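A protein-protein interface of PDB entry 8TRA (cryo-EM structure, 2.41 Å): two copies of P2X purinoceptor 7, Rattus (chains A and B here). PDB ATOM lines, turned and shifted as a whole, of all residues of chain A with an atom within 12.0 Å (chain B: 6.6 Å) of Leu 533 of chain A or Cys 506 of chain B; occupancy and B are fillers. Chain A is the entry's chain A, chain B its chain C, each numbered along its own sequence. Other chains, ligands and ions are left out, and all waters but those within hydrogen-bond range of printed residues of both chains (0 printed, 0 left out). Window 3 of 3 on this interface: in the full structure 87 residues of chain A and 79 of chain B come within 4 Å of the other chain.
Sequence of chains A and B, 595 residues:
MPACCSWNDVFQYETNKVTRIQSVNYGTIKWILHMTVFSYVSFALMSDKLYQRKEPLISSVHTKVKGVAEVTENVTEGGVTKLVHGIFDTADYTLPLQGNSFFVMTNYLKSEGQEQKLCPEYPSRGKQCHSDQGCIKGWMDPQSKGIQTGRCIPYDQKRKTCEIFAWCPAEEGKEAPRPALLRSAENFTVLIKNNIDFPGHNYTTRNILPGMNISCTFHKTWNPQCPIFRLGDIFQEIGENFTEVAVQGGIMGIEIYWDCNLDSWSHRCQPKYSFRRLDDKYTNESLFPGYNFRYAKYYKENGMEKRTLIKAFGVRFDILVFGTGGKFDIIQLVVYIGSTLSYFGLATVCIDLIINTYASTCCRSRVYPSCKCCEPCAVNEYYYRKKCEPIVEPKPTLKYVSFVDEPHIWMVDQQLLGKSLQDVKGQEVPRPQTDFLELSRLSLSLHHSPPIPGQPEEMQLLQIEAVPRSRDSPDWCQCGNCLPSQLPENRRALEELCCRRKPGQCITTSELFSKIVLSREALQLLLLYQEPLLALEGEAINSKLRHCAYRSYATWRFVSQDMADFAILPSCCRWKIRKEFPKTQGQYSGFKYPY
No position is printed for both chains.
Of the 18 printed residues of chain B, 5 touch a printed residue of chain A. Hydrophobic or aromatic side chains of chain B that line the printed part of chain A: Val 404. Of the 18 printed residues of chain A, 2 touch a printed residue of chain B. Printed residues of chain A that touch a printed residue of chain B: Pro 532 and Leu 533.
Of the printed residues of chain B, Pro 532 of chain A touches Ser 510. Leu 533 of chain A touches just these residues of chain B: Val 404 (3.6 Å), Arg 500 (3.6 Å), Gln 505 (3.6 Å) and Cys 506 (3.98 Å). Val 404 of chain B touches just one residue of chain A: Leu 533 (3.6 Å). No residue of chain A comes within 4 Å of Cys 479 of chain B. No residue of chain A comes within 4 Å of Gly 480 of chain B. Cys 499 of chain B touches none of the printed residues of chain A. Printed residues of chain A within 4 Å of Arg 500 of chain B: Leu 533 (3.6 Å). Of chain A, only Leu 533 comes within 4 Å of Gln 505 of chain B. Ser 510 of chain B touches just one residue of chain A: Pro 532. No residue of chain A comes within 4 Å of Cys 572 of chain B. The nearest printed residue of chain B that does not touch Pro 532 of chain A is Ile 507 of chain B (4.03 Å).
O of Pro 532 of chain A touches CB of Ser 510 of chain B, 3.6 Å away. Leu 533 of chain A touches Val 404 of chain B. Leu 533 of chain A touches Arg 500 of chain B (CD1 to NH1, 3.6 Å). Leu 533 of chain A touches Gln 505 of chain B (CD1 to O, 3.6 Å). Leu 533 of chain A touches Cys 506 of chain B (CD2 to O, 3.98 Å).
The backbone NH (N) of Val 404 of chain B is in hydrogen-bond range of the backbone carbonyl oxygen (O) of Cys 499 of chain B. OE1 of Gln 478 of chain B lies close to O of Arg 500 of chain B, 3.0 Å away. The side-chain amide oxygen of Asn 481 of chain B sits close to the side-chain sulfur of Cys 506 of chain B, at 3.8 Å. OE1 of Gln 505 of chain B lies within hydrogen-bond range of OG1 of Thr 509 of chain B (3.2 Å). OG1 of Thr 508 of chain B lies close to SG of Cys 506 of chain B, 2.9 Å away. The backbone carbonyl oxygen of Cys 506 of chain B sits at hydrogen-bond distance from the side-chain hydroxyl of Thr 509 of chain B (2.6 Å).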
ATOM      1  N   LEU A 523      19.952 -16.916   8.974  1.00  0.00           N
ATOM      2  CA  LEU A 523      19.651 -15.754   8.145  1.00  0.00           C
ATOM      3  C   LEU A 523      18.340 -15.946   7.393  1.00  0.00           C
ATOM      4  O   LEU A 523      17.544 -15.006   7.267  1.00  0.00           O
ATOM      5  CB  LEU A 523      20.799 -15.492   7.172  1.00  0.00           C
ATOM      6  CG  LEU A 523      22.187 -15.338   7.797  1.00  0.00           C
ATOM      7  CD1 LEU A 523      23.232 -15.135   6.714  1.00  0.00           C
ATOM      8  CD2 LEU A 523      22.215 -14.191   8.794  1.00  0.00           C
ATOM      9  N   GLN A 524      18.100 -17.155   6.885  1.00  0.00           N
ATOM     10  CA  GLN A 524      16.830 -17.433   6.221  1.00  0.00           C
ATOM     11  C   GLN A 524      15.666 -17.286   7.192  1.00  0.00           C
ATOM     12  O   GLN A 524      14.612 -16.755   6.828  1.00  0.00           O
ATOM     13  CB  GLN A 524      16.851 -18.836   5.616  1.00  0.00           C
ATOM     14  CG  GLN A 524      17.235 -18.865   4.140  1.00  0.00           C
ATOM     15  CD  GLN A 524      17.939 -20.149   3.713  1.00  0.00           C
ATOM     16  OE1 GLN A 524      17.856 -21.164   4.404  1.00  0.00           O
ATOM     17  NE2 GLN A 524      18.655 -20.105   2.591  1.00  0.00           N
ATOM     18  N   LEU A 525      15.833 -17.759   8.427  1.00  0.00           N
ATOM     19  CA  LEU A 525      14.781 -17.608   9.426  1.00  0.00           C
ATOM     20  C   LEU A 525      14.495 -16.139   9.699  1.00  0.00           C
ATOM     21  O   LEU A 525      13.331 -15.731   9.791  1.00  0.00           O
ATOM     22  CB  LEU A 525      15.182 -18.324  10.716  1.00  0.00           C
ATOM     23  CG  LEU A 525      15.084 -19.854  10.747  1.00  0.00           C
ATOM     24  CD1 LEU A 525      15.454 -20.366  12.128  1.00  0.00           C
ATOM     25  CD2 LEU A 525      13.700 -20.350  10.357  1.00  0.00           C
ATOM     26  N   LEU A 526      15.545 -15.327   9.830  1.00  0.00           N
ATOM     27  CA  LEU A 526      15.351 -13.896  10.052  1.00  0.00           C
ATOM     28  C   LEU A 526      14.617 -13.258   8.879  1.00  0.00           C
ATOM     29  O   LEU A 526      13.675 -12.474   9.067  1.00  0.00           O
ATOM     30  CB  LEU A 526      16.703 -13.216  10.273  1.00  0.00           C
ATOM     31  CG  LEU A 526      17.194 -13.102  11.718  1.00  0.00           C
ATOM     32  CD1 LEU A 526      16.890 -14.364  12.510  1.00  0.00           C
ATOM     33  CD2 LEU A 526      18.684 -12.800  11.743  1.00  0.00           C
ATOM     34  N   LEU A 527      15.031 -13.588   7.653  1.00  0.00           N
ATOM     35  CA  LEU A 527      14.393 -13.007   6.477  1.00  0.00           C
ATOM     36  C   LEU A 527      12.928 -13.415   6.386  1.00  0.00           C
ATOM     37  O   LEU A 527      12.068 -12.595   6.047  1.00  0.00           O
ATOM     38  CB  LEU A 527      15.148 -13.420   5.215  1.00  0.00           C
ATOM     39  CG  LEU A 527      16.591 -12.917   5.122  1.00  0.00           C
ATOM     40  CD1 LEU A 527      17.372 -13.711   4.087  1.00  0.00           C
ATOM     41  CD2 LEU A 527      16.622 -11.434   4.798  1.00  0.00           C
ATOM     42  N   LEU A 528      12.624 -14.681   6.682  1.00  0.00           N
ATOM     43  CA  LEU A 528      11.235 -15.125   6.685  1.00  0.00           C
ATOM     44  C   LEU A 528      10.437 -14.406   7.764  1.00  0.00           C
ATOM     45  O   LEU A 528       9.276 -14.041   7.549  1.00  0.00           O
ATOM     46  CB  LEU A 528      11.164 -16.639   6.879  1.00  0.00           C
ATOM     47  CG  LEU A 528      11.919 -17.481   5.847  1.00  0.00           C
ATOM     48  CD1 LEU A 528      12.381 -18.795   6.454  1.00  0.00           C
ATOM     49  CD2 LEU A 528      11.054 -17.732   4.624  1.00  0.00           C
ATOM     50  N   TYR A 529      11.044 -14.193   8.935  1.00  0.00           N
ATOM     51  CA  TYR A 529      10.381 -13.409   9.969  1.00  0.00           C
ATOM     52  C   TYR A 529      10.033 -12.021   9.453  1.00  0.00           C
ATOM     53  O   TYR A 529       8.936 -11.512   9.706  1.00  0.00           O
ATOM     54  CB  TYR A 529      11.275 -13.316  11.207  1.00  0.00           C
ATOM     55  CG  TYR A 529      10.560 -12.837  12.450  1.00  0.00           C
ATOM     56  CD1 TYR A 529      10.365 -11.482  12.686  1.00  0.00           C
ATOM     57  CD2 TYR A 529      10.084 -13.740  13.391  1.00  0.00           C
ATOM     58  CE1 TYR A 529       9.715 -11.042  13.822  1.00  0.00           C
ATOM     59  CE2 TYR A 529       9.432 -13.308  14.530  1.00  0.00           C
ATOM     60  CZ  TYR A 529       9.250 -11.959  14.740  1.00  0.00           C
ATOM     61  OH  TYR A 529       8.602 -11.524  15.872  1.00  0.00           O
ATOM     62  N   GLN A 530      10.958 -11.393   8.723  1.00  0.00           N
ATOM     63  CA  GLN A 530      10.654 -10.107   8.106  1.00  0.00           C
ATOM     64  C   GLN A 530       9.743 -10.265   6.891  1.00  0.00           C
ATOM     65  O   GLN A 530       8.819  -9.467   6.699  1.00  0.00           O
ATOM     66  CB  GLN A 530      11.948  -9.396   7.711  1.00  0.00           C
ATOM     67  CG  GLN A 530      12.576  -8.583   8.833  1.00  0.00           C
ATOM     68  CD  GLN A 530      13.611  -9.368   9.614  1.00  0.00           C
ATOM     69  OE1 GLN A 530      13.404  -9.701  10.780  1.00  0.00           O
ATOM     70  NE2 GLN A 530      14.736  -9.666   8.974  1.00  0.00           N
ATOM     71  N   GLU A 531       9.986 -11.285   6.066  1.00  0.00           N
ATOM     72  CA  GLU A 531       9.221 -11.524   4.840  1.00  0.00           C
ATOM     73  C   GLU A 531       8.760 -12.975   4.825  1.00  0.00           C
ATOM     74  O   GLU A 531       9.459 -13.852   4.302  1.00  0.00           O
ATOM     75  CB  GLU A 531      10.053 -11.200   3.601  1.00  0.00           C
ATOM     76  CG  GLU A 531       9.842  -9.791   3.070  1.00  0.00           C
ATOM     77  CD  GLU A 531      10.837  -9.423   1.987  1.00  0.00           C
ATOM     78  OE1 GLU A 531      12.055  -9.481   2.253  1.00  0.00           O
ATOM     79  OE2 GLU A 531      10.400  -9.075   0.870  1.00  0.00           O
ATOM     80  N   PRO A 532       7.578 -13.267   5.381  1.00  0.00           N
ATOM     81  CA  PRO A 532       7.169 -14.678   5.514  1.00  0.00           C
ATOM     82  C   PRO A 532       7.157 -15.444   4.203  1.00  0.00           C
ATOM     83  O   PRO A 532       7.521 -16.627   4.184  1.00  0.00           O
ATOM     84  CB  PRO A 532       5.761 -14.576   6.123  1.00  0.00           C
ATOM     85  CG  PRO A 532       5.695 -13.223   6.740  1.00  0.00           C
ATOM     86  CD  PRO A 532       6.564 -12.341   5.912  1.00  0.00           C
ATOM     87  N   LEU A 533       6.751 -14.810   3.103  1.00  0.00           N
ATOM     88  CA  LEU A 533       6.648 -15.469   1.807  1.00  0.00           C
ATOM     89  C   LEU A 533       7.826 -15.138   0.894  1.00  0.00           C
ATOM     90  O   LEU A 533       7.658 -15.031  -0.324  1.00  0.00           O
ATOM     91  CB  LEU A 533       5.331 -15.096   1.128  1.00  0.00           C
ATOM     92  CG  LEU A 533       4.064 -15.396   1.932  1.00  0.00           C
ATOM     93  CD1 LEU A 533       2.831 -14.929   1.175  1.00  0.00           C
ATOM     94  CD2 LEU A 533       3.963 -16.877   2.264  1.00  0.00           C
ATOM     95  N   LEU A 534       9.016 -14.972   1.463  1.00  0.00           N
ATOM     96  CA  LEU A 534      10.191 -14.652   0.662  1.00  0.00           C
ATOM     97  C   LEU A 534      10.565 -15.823  -0.236  1.00  0.00           C
ATOM     98  O   LEU A 534      10.421 -16.989   0.141  1.00  0.00           O
ATOM     99  CB  LEU A 534      11.366 -14.290   1.570  1.00  0.00           C
ATOM    100  CG  LEU A 534      12.622 -13.773   0.865  1.00  0.00           C
ATOM    101  CD1 LEU A 534      12.347 -12.448   0.173  1.00  0.00           C
ATOM    102  CD2 LEU A 534      13.764 -13.633   1.856  1.00  0.00           C
ATOM    103  N   ALA A 535      11.051 -15.504  -1.435  1.00  0.00           N
ATOM    104  CA  ALA A 535      11.489 -16.510  -2.397  1.00  0.00           C
ATOM    105  C   ALA A 535      12.979 -16.757  -2.196  1.00  0.00           C
ATOM    106  O   ALA A 535      13.800 -15.861  -2.413  1.00  0.00           O
ATOM    107  CB  ALA A 535      11.193 -16.055  -3.823  1.00  0.00           C
ATOM    108  N   LEU A 536      13.329 -17.976  -1.783  1.00  0.00           N
ATOM    109  CA  LEU A 536      14.721 -18.335  -1.507  1.00  0.00           C
ATOM    110  C   LEU A 536      15.375 -18.869  -2.784  1.00  0.00           C
ATOM    111  O   LEU A 536      15.687 -20.053  -2.924  1.00  0.00           O
ATOM    112  CB  LEU A 536      14.791 -19.351  -0.373  1.00  0.00           C
ATOM    113  CG  LEU A 536      13.849 -19.122   0.812  1.00  0.00           C
ATOM    114  CD1 LEU A 536      13.851 -20.328   1.738  1.00  0.00           C
ATOM    115  CD2 LEU A 536      14.228 -17.862   1.571  1.00  0.00           C
ATOM    116  N   GLU A 537      15.582 -17.956  -3.731  1.00  0.00           N
ATOM    117  CA  GLU A 537      16.199 -18.311  -5.001  1.00  0.00           C
ATOM    118  C   GLU A 537      16.812 -17.065  -5.623  1.00  0.00           C
ATOM    119  O   GLU A 537      16.449 -15.935  -5.285  1.00  0.00           O
ATOM    120  CB  GLU A 537      15.185 -18.946  -5.958  1.00  0.00           C
ATOM    121  N   ALA A 540      19.302 -12.444  -5.574  1.00  0.00           N
ATOM    122  CA  ALA A 540      18.676 -11.530  -4.625  1.00  0.00           C
ATOM    123  C   ALA A 540      18.707 -12.103  -3.216  1.00  0.00           C
ATOM    124  O   ALA A 540      18.961 -11.378  -2.247  1.00  0.00           O
ATOM    125  CB  ALA A 540      17.241 -11.232  -5.053  1.00  0.00           C
ATOM    126  N   ILE A 541      18.449 -13.406  -3.080  1.00  0.00           N
ATOM    127  CA  ILE A 541      18.518 -14.032  -1.764  1.00  0.00           C
ATOM    128  C   ILE A 541      19.945 -13.997  -1.239  1.00  0.00           C
ATOM    129  O   ILE A 541      20.173 -13.842  -0.037  1.00  0.00           O
ATOM    130  CB  ILE A 541      17.962 -15.469  -1.818  1.00  0.00           C
ATOM    131  CG1 ILE A 541      17.463 -15.896  -0.436  1.00  0.00           C
ATOM    132  CG2 ILE A 541      19.024 -16.446  -2.300  1.00  0.00           C
ATOM    133  CD1 ILE A 541      16.173 -15.226  -0.014  1.00  0.00           C
ATOM    134  N   LYS A 544      20.482 -10.472   0.055  1.00  0.00           N
ATOM    135  CA  LYS A 544      19.747 -10.347   1.309  1.00  0.00           C
ATOM    136  C   LYS A 544      20.476 -11.053   2.447  1.00  0.00           C
ATOM    137  O   LYS A 544      20.580 -10.516   3.554  1.00  0.00           O
ATOM    138  CB  LYS A 544      18.338 -10.914   1.128  1.00  0.00           C
ATOM    139  CG  LYS A 544      17.356 -10.000   0.386  1.00  0.00           C
ATOM    140  CD  LYS A 544      15.976 -10.667   0.315  1.00  0.00           C
ATOM    141  CE  LYS A 544      14.748  -9.774   0.584  1.00  0.00           C
ATOM    142  NZ  LYS A 544      14.933  -8.305   0.791  1.00  0.00           N
ATOM    143  N   VAL B 404       0.115  -9.911   4.238  1.00  0.00           N
ATOM    144  CA  VAL B 404       1.435 -10.436   3.901  1.00  0.00           C
ATOM    145  C   VAL B 404       1.960  -9.781   2.630  1.00  0.00           C
ATOM    146  O   VAL B 404       3.158  -9.495   2.509  1.00  0.00           O
ATOM    147  CB  VAL B 404       1.384 -11.970   3.777  1.00  0.00           C
ATOM    148  CG1 VAL B 404       0.709 -12.386   2.477  1.00  0.00           C
ATOM    149  CG2 VAL B 404       2.782 -12.556   3.875  1.00  0.00           C
ATOM    150  N   ASP B 405       1.077  -9.535   1.660  1.00  0.00           N
ATOM    151  CA  ASP B 405       1.503  -8.874   0.431  1.00  0.00           C
ATOM    152  C   ASP B 405       1.980  -7.453   0.708  1.00  0.00           C
ATOM    153  O   ASP B 405       3.004  -7.017   0.166  1.00  0.00           O
ATOM    154  CB  ASP B 405       0.361  -8.867  -0.588  1.00  0.00           C
ATOM    155  CG  ASP B 405      -0.918  -8.283  -0.025  1.00  0.00           C
ATOM    156  OD1 ASP B 405      -1.576  -8.966   0.787  1.00  0.00           O
ATOM    157  OD2 ASP B 405      -1.266  -7.142  -0.395  1.00  0.00           O
ATOM    158  N   GLN B 478      -8.812 -14.060  -0.132  1.00  0.00           N
ATOM    159  CA  GLN B 478      -7.897 -14.112  -1.267  1.00  0.00           C
ATOM    160  C   GLN B 478      -6.805 -15.156  -1.066  1.00  0.00           C
ATOM    161  O   GLN B 478      -5.763 -15.096  -1.725  1.00  0.00           O
ATOM    162  CB  GLN B 478      -7.277 -12.734  -1.511  1.00  0.00           C
ATOM    163  CG  GLN B 478      -8.101 -11.826  -2.414  1.00  0.00           C
ATOM    164  CD  GLN B 478      -8.756 -10.684  -1.662  1.00  0.00           C
ATOM    165  OE1 GLN B 478      -8.168 -10.112  -0.743  1.00  0.00           O
ATOM    166  NE2 GLN B 478      -9.978 -10.345  -2.052  1.00  0.00           N
ATOM    167  N   CYS B 479      -7.024 -16.116  -0.168  1.00  0.00           N
ATOM    168  CA  CYS B 479      -6.032 -17.144   0.125  1.00  0.00           C
ATOM    169  C   CYS B 479      -6.579 -18.563   0.091  1.00  0.00           C
ATOM    170  O   CYS B 479      -5.778 -19.506   0.047  1.00  0.00           O
ATOM    171  CB  CYS B 479      -5.397 -16.894   1.502  1.00  0.00           C
ATOM    172  SG  CYS B 479      -6.347 -17.536   2.898  1.00  0.00           S
ATOM    173  N   GLY B 480      -7.897 -18.754   0.108  1.00  0.00           N
ATOM    174  CA  GLY B 480      -8.481 -20.073   0.000  1.00  0.00           C
ATOM    175  C   GLY B 480      -8.518 -20.875   1.281  1.00  0.00           C
ATOM    176  O   GLY B 480      -8.945 -22.037   1.249  1.00  0.00           O
ATOM    177  N   ASN B 481      -8.087 -20.304   2.405  1.00  0.00           N
ATOM    178  CA  ASN B 481      -8.078 -21.004   3.682  1.00  0.00           C
ATOM    179  C   ASN B 481      -8.969 -20.353   4.729  1.00  0.00           C
ATOM    180  O   ASN B 481      -9.121 -20.912   5.822  1.00  0.00           O
ATOM    181  CB  ASN B 481      -6.644 -21.098   4.222  1.00  0.00           C
ATOM    182  CG  ASN B 481      -5.714 -21.836   3.281  1.00  0.00           C
ATOM    183  OD1 ASN B 481      -4.870 -21.229   2.621  1.00  0.00           O
ATOM    184  ND2 ASN B 481      -5.865 -23.154   3.211  1.00  0.00           N
ATOM    185  N   CYS B 482      -9.557 -19.199   4.435  1.00  0.00           N
ATOM    186  CA  CYS B 482     -10.426 -18.531   5.389  1.00  0.00           C
ATOM    187  C   CYS B 482     -11.805 -19.184   5.410  1.00  0.00           C
ATOM    188  O   CYS B 482     -12.226 -19.843   4.456  1.00  0.00           O
ATOM    189  CB  CYS B 482     -10.554 -17.047   5.049  1.00  0.00           C
ATOM    190  SG  CYS B 482      -9.019 -16.112   5.237  1.00  0.00           S
ATOM    191  N   CYS B 499      -5.638 -12.899   5.042  1.00  0.00           N
ATOM    192  CA  CYS B 499      -4.219 -12.644   5.251  1.00  0.00           C
ATOM    193  C   CYS B 499      -3.608 -11.758   4.175  1.00  0.00           C
ATOM    194  O   CYS B 499      -2.472 -11.305   4.348  1.00  0.00           O
ATOM    195  CB  CYS B 499      -3.458 -13.971   5.309  1.00  0.00           C
ATOM    196  SG  CYS B 499      -3.651 -14.999   3.836  1.00  0.00           S
ATOM    197  N   ARG B 500      -4.320 -11.501   3.080  1.00  0.00           N
ATOM    198  CA  ARG B 500      -3.765 -10.724   1.981  1.00  0.00           C
ATOM    199  C   ARG B 500      -4.881  -9.954   1.293  1.00  0.00           C
ATOM    200  O   ARG B 500      -6.064 -10.280   1.422  1.00  0.00           O
ATOM    201  CB  ARG B 500      -3.040 -11.620   0.971  1.00  0.00           C
ATOM    202  CG  ARG B 500      -3.779 -12.907   0.633  1.00  0.00           C
ATOM    203  CD  ARG B 500      -2.936 -13.828  -0.236  1.00  0.00           C
ATOM    204  NE  ARG B 500      -2.005 -13.084  -1.077  1.00  0.00           N
ATOM    205  CZ  ARG B 500      -0.729 -13.398  -1.264  1.00  0.00           C
ATOM    206  NH1 ARG B 500      -0.183 -14.460  -0.694  1.00  0.00           N
ATOM    207  NH2 ARG B 500       0.019 -12.624  -2.047  1.00  0.00           N
ATOM    208  N   GLY B 504      -3.345 -15.134  -3.781  1.00  0.00           N
ATOM    209  CA  GLY B 504      -1.998 -15.660  -3.650  1.00  0.00           C
ATOM    210  C   GLY B 504      -1.957 -16.767  -2.613  1.00  0.00           C
ATOM    211  O   GLY B 504      -2.991 -17.327  -2.244  1.00  0.00           O
ATOM    212  N   GLN B 505      -0.744 -17.069  -2.157  1.00  0.00           N
ATOM    213  CA  GLN B 505      -0.547 -18.132  -1.180  1.00  0.00           C
ATOM    214  C   GLN B 505      -0.780 -17.608   0.233  1.00  0.00           C
ATOM    215  O   GLN B 505      -0.374 -16.495   0.576  1.00  0.00           O
ATOM    216  CB  GLN B 505       0.863 -18.713  -1.294  1.00  0.00           C
ATOM    217  CG  GLN B 505       1.972 -17.675  -1.363  1.00  0.00           C
ATOM    218  CD  GLN B 505       3.334 -18.250  -1.031  1.00  0.00           C
ATOM    219  OE1 GLN B 505       3.440 -19.325  -0.440  1.00  0.00           O
ATOM    220  NE2 GLN B 505       4.386 -17.534  -1.409  1.00  0.00           N
ATOM    221  N   CYS B 506      -1.441 -18.425   1.049  1.00  0.00           N
ATOM    222  CA  CYS B 506      -1.734 -18.040   2.421  1.00  0.00           C
ATOM    223  C   CYS B 506      -0.457 -17.970   3.250  1.00  0.00           C
ATOM    224  O   CYS B 506       0.507 -18.703   3.013  1.00  0.00           O
ATOM    225  CB  CYS B 506      -2.709 -19.035   3.054  1.00  0.00           C
ATOM    226  SG  CYS B 506      -3.182 -18.642   4.751  1.00  0.00           S
ATOM    227  N   ILE B 507      -0.459 -17.066   4.233  1.00  0.00           N
ATOM    228  CA  ILE B 507       0.688 -16.938   5.125  1.00  0.00           C
ATOM    229  C   ILE B 507       0.896 -18.220   5.921  1.00  0.00           C
ATOM    230  O   ILE B 507       2.015 -18.514   6.358  1.00  0.00           O
ATOM    231  CB  ILE B 507       0.507 -15.723   6.058  1.00  0.00           C
ATOM    232  CG1 ILE B 507       1.811 -15.425   6.801  1.00  0.00           C
ATOM    233  CG2 ILE B 507      -0.620 -15.977   7.048  1.00  0.00           C
ATOM    234  CD1 ILE B 507       1.825 -14.079   7.489  1.00  0.00           C
ATOM    235  N   THR B 508      -0.169 -18.998   6.126  1.00  0.00           N
ATOM    236  CA  THR B 508      -0.042 -20.241   6.876  1.00  0.00           C
ATOM    237  C   THR B 508       0.895 -21.221   6.186  1.00  0.00           C
ATOM    238  O   THR B 508       1.503 -22.072   6.847  1.00  0.00           O
ATOM    239  CB  THR B 508      -1.417 -20.884   7.067  1.00  0.00           C
ATOM    240  OG1 THR B 508      -2.013 -21.141   5.790  1.00  0.00           O
ATOM    241  CG2 THR B 508      -2.331 -19.975   7.879  1.00  0.00           C
ATOM    242  N   THR B 509       1.028 -21.124   4.860  1.00  0.00           N
ATOM    243  CA  THR B 509       1.896 -22.039   4.131  1.00  0.00           C
ATOM    244  C   THR B 509       3.358 -21.885   4.529  1.00  0.00           C
ATOM    245  O   THR B 509       4.136 -22.832   4.364  1.00  0.00           O
ATOM    246  CB  THR B 509       1.747 -21.819   2.624  1.00  0.00           C
ATOM    247  OG1 THR B 509       2.219 -20.511   2.279  1.00  0.00           O
ATOM    248  CG2 THR B 509       0.291 -21.958   2.203  1.00  0.00           C
ATOM    249  N   SER B 510       3.746 -20.725   5.044  1.00  0.00           N
ATOM    250  CA  SER B 510       5.126 -20.514   5.461  1.00  0.00           C
ATOM    251  C   SER B 510       5.461 -21.394   6.659  1.00  0.00           C
ATOM    252  O   SER B 510       4.631 -21.609   7.545  1.00  0.00           O
ATOM    253  CB  SER B 510       5.355 -19.045   5.807  1.00  0.00           C
ATOM    254  OG  SER B 510       4.571 -18.653   6.919  1.00  0.00           O
ATOM    255  N   CYS B 572      -8.100 -17.231   8.248  1.00  0.00           N
ATOM    256  CA  CYS B 572      -7.341 -18.446   7.965  1.00  0.00           C
ATOM    257  C   CYS B 572      -6.453 -18.826   9.144  1.00  0.00           C
ATOM    258  O   CYS B 572      -6.497 -19.961   9.631  1.00  0.00           O
ATOM    259  CB  CYS B 572      -6.497 -18.249   6.706  1.00  0.00           C
ATOM    260  SG  CYS B 572      -5.835 -16.576   6.520  1.00  0.00           S
ATOM    261  N   CYS B 573      -5.638 -17.880   9.619  1.00  0.00           N
ATOM    262  CA  CYS B 573      -4.733 -18.169  10.727  1.00  0.00           C
ATOM    263  C   CYS B 573      -5.503 -18.449  12.011  1.00  0.00           C
ATOM    264  O   CYS B 573      -5.147 -19.360  12.769  1.00  0.00           O
ATOM    265  CB  CYS B 573      -3.768 -17.002  10.923  1.00  0.00           C
ATOM    266  SG  CYS B 573      -3.028 -16.400   9.388  1.00  0.00           S
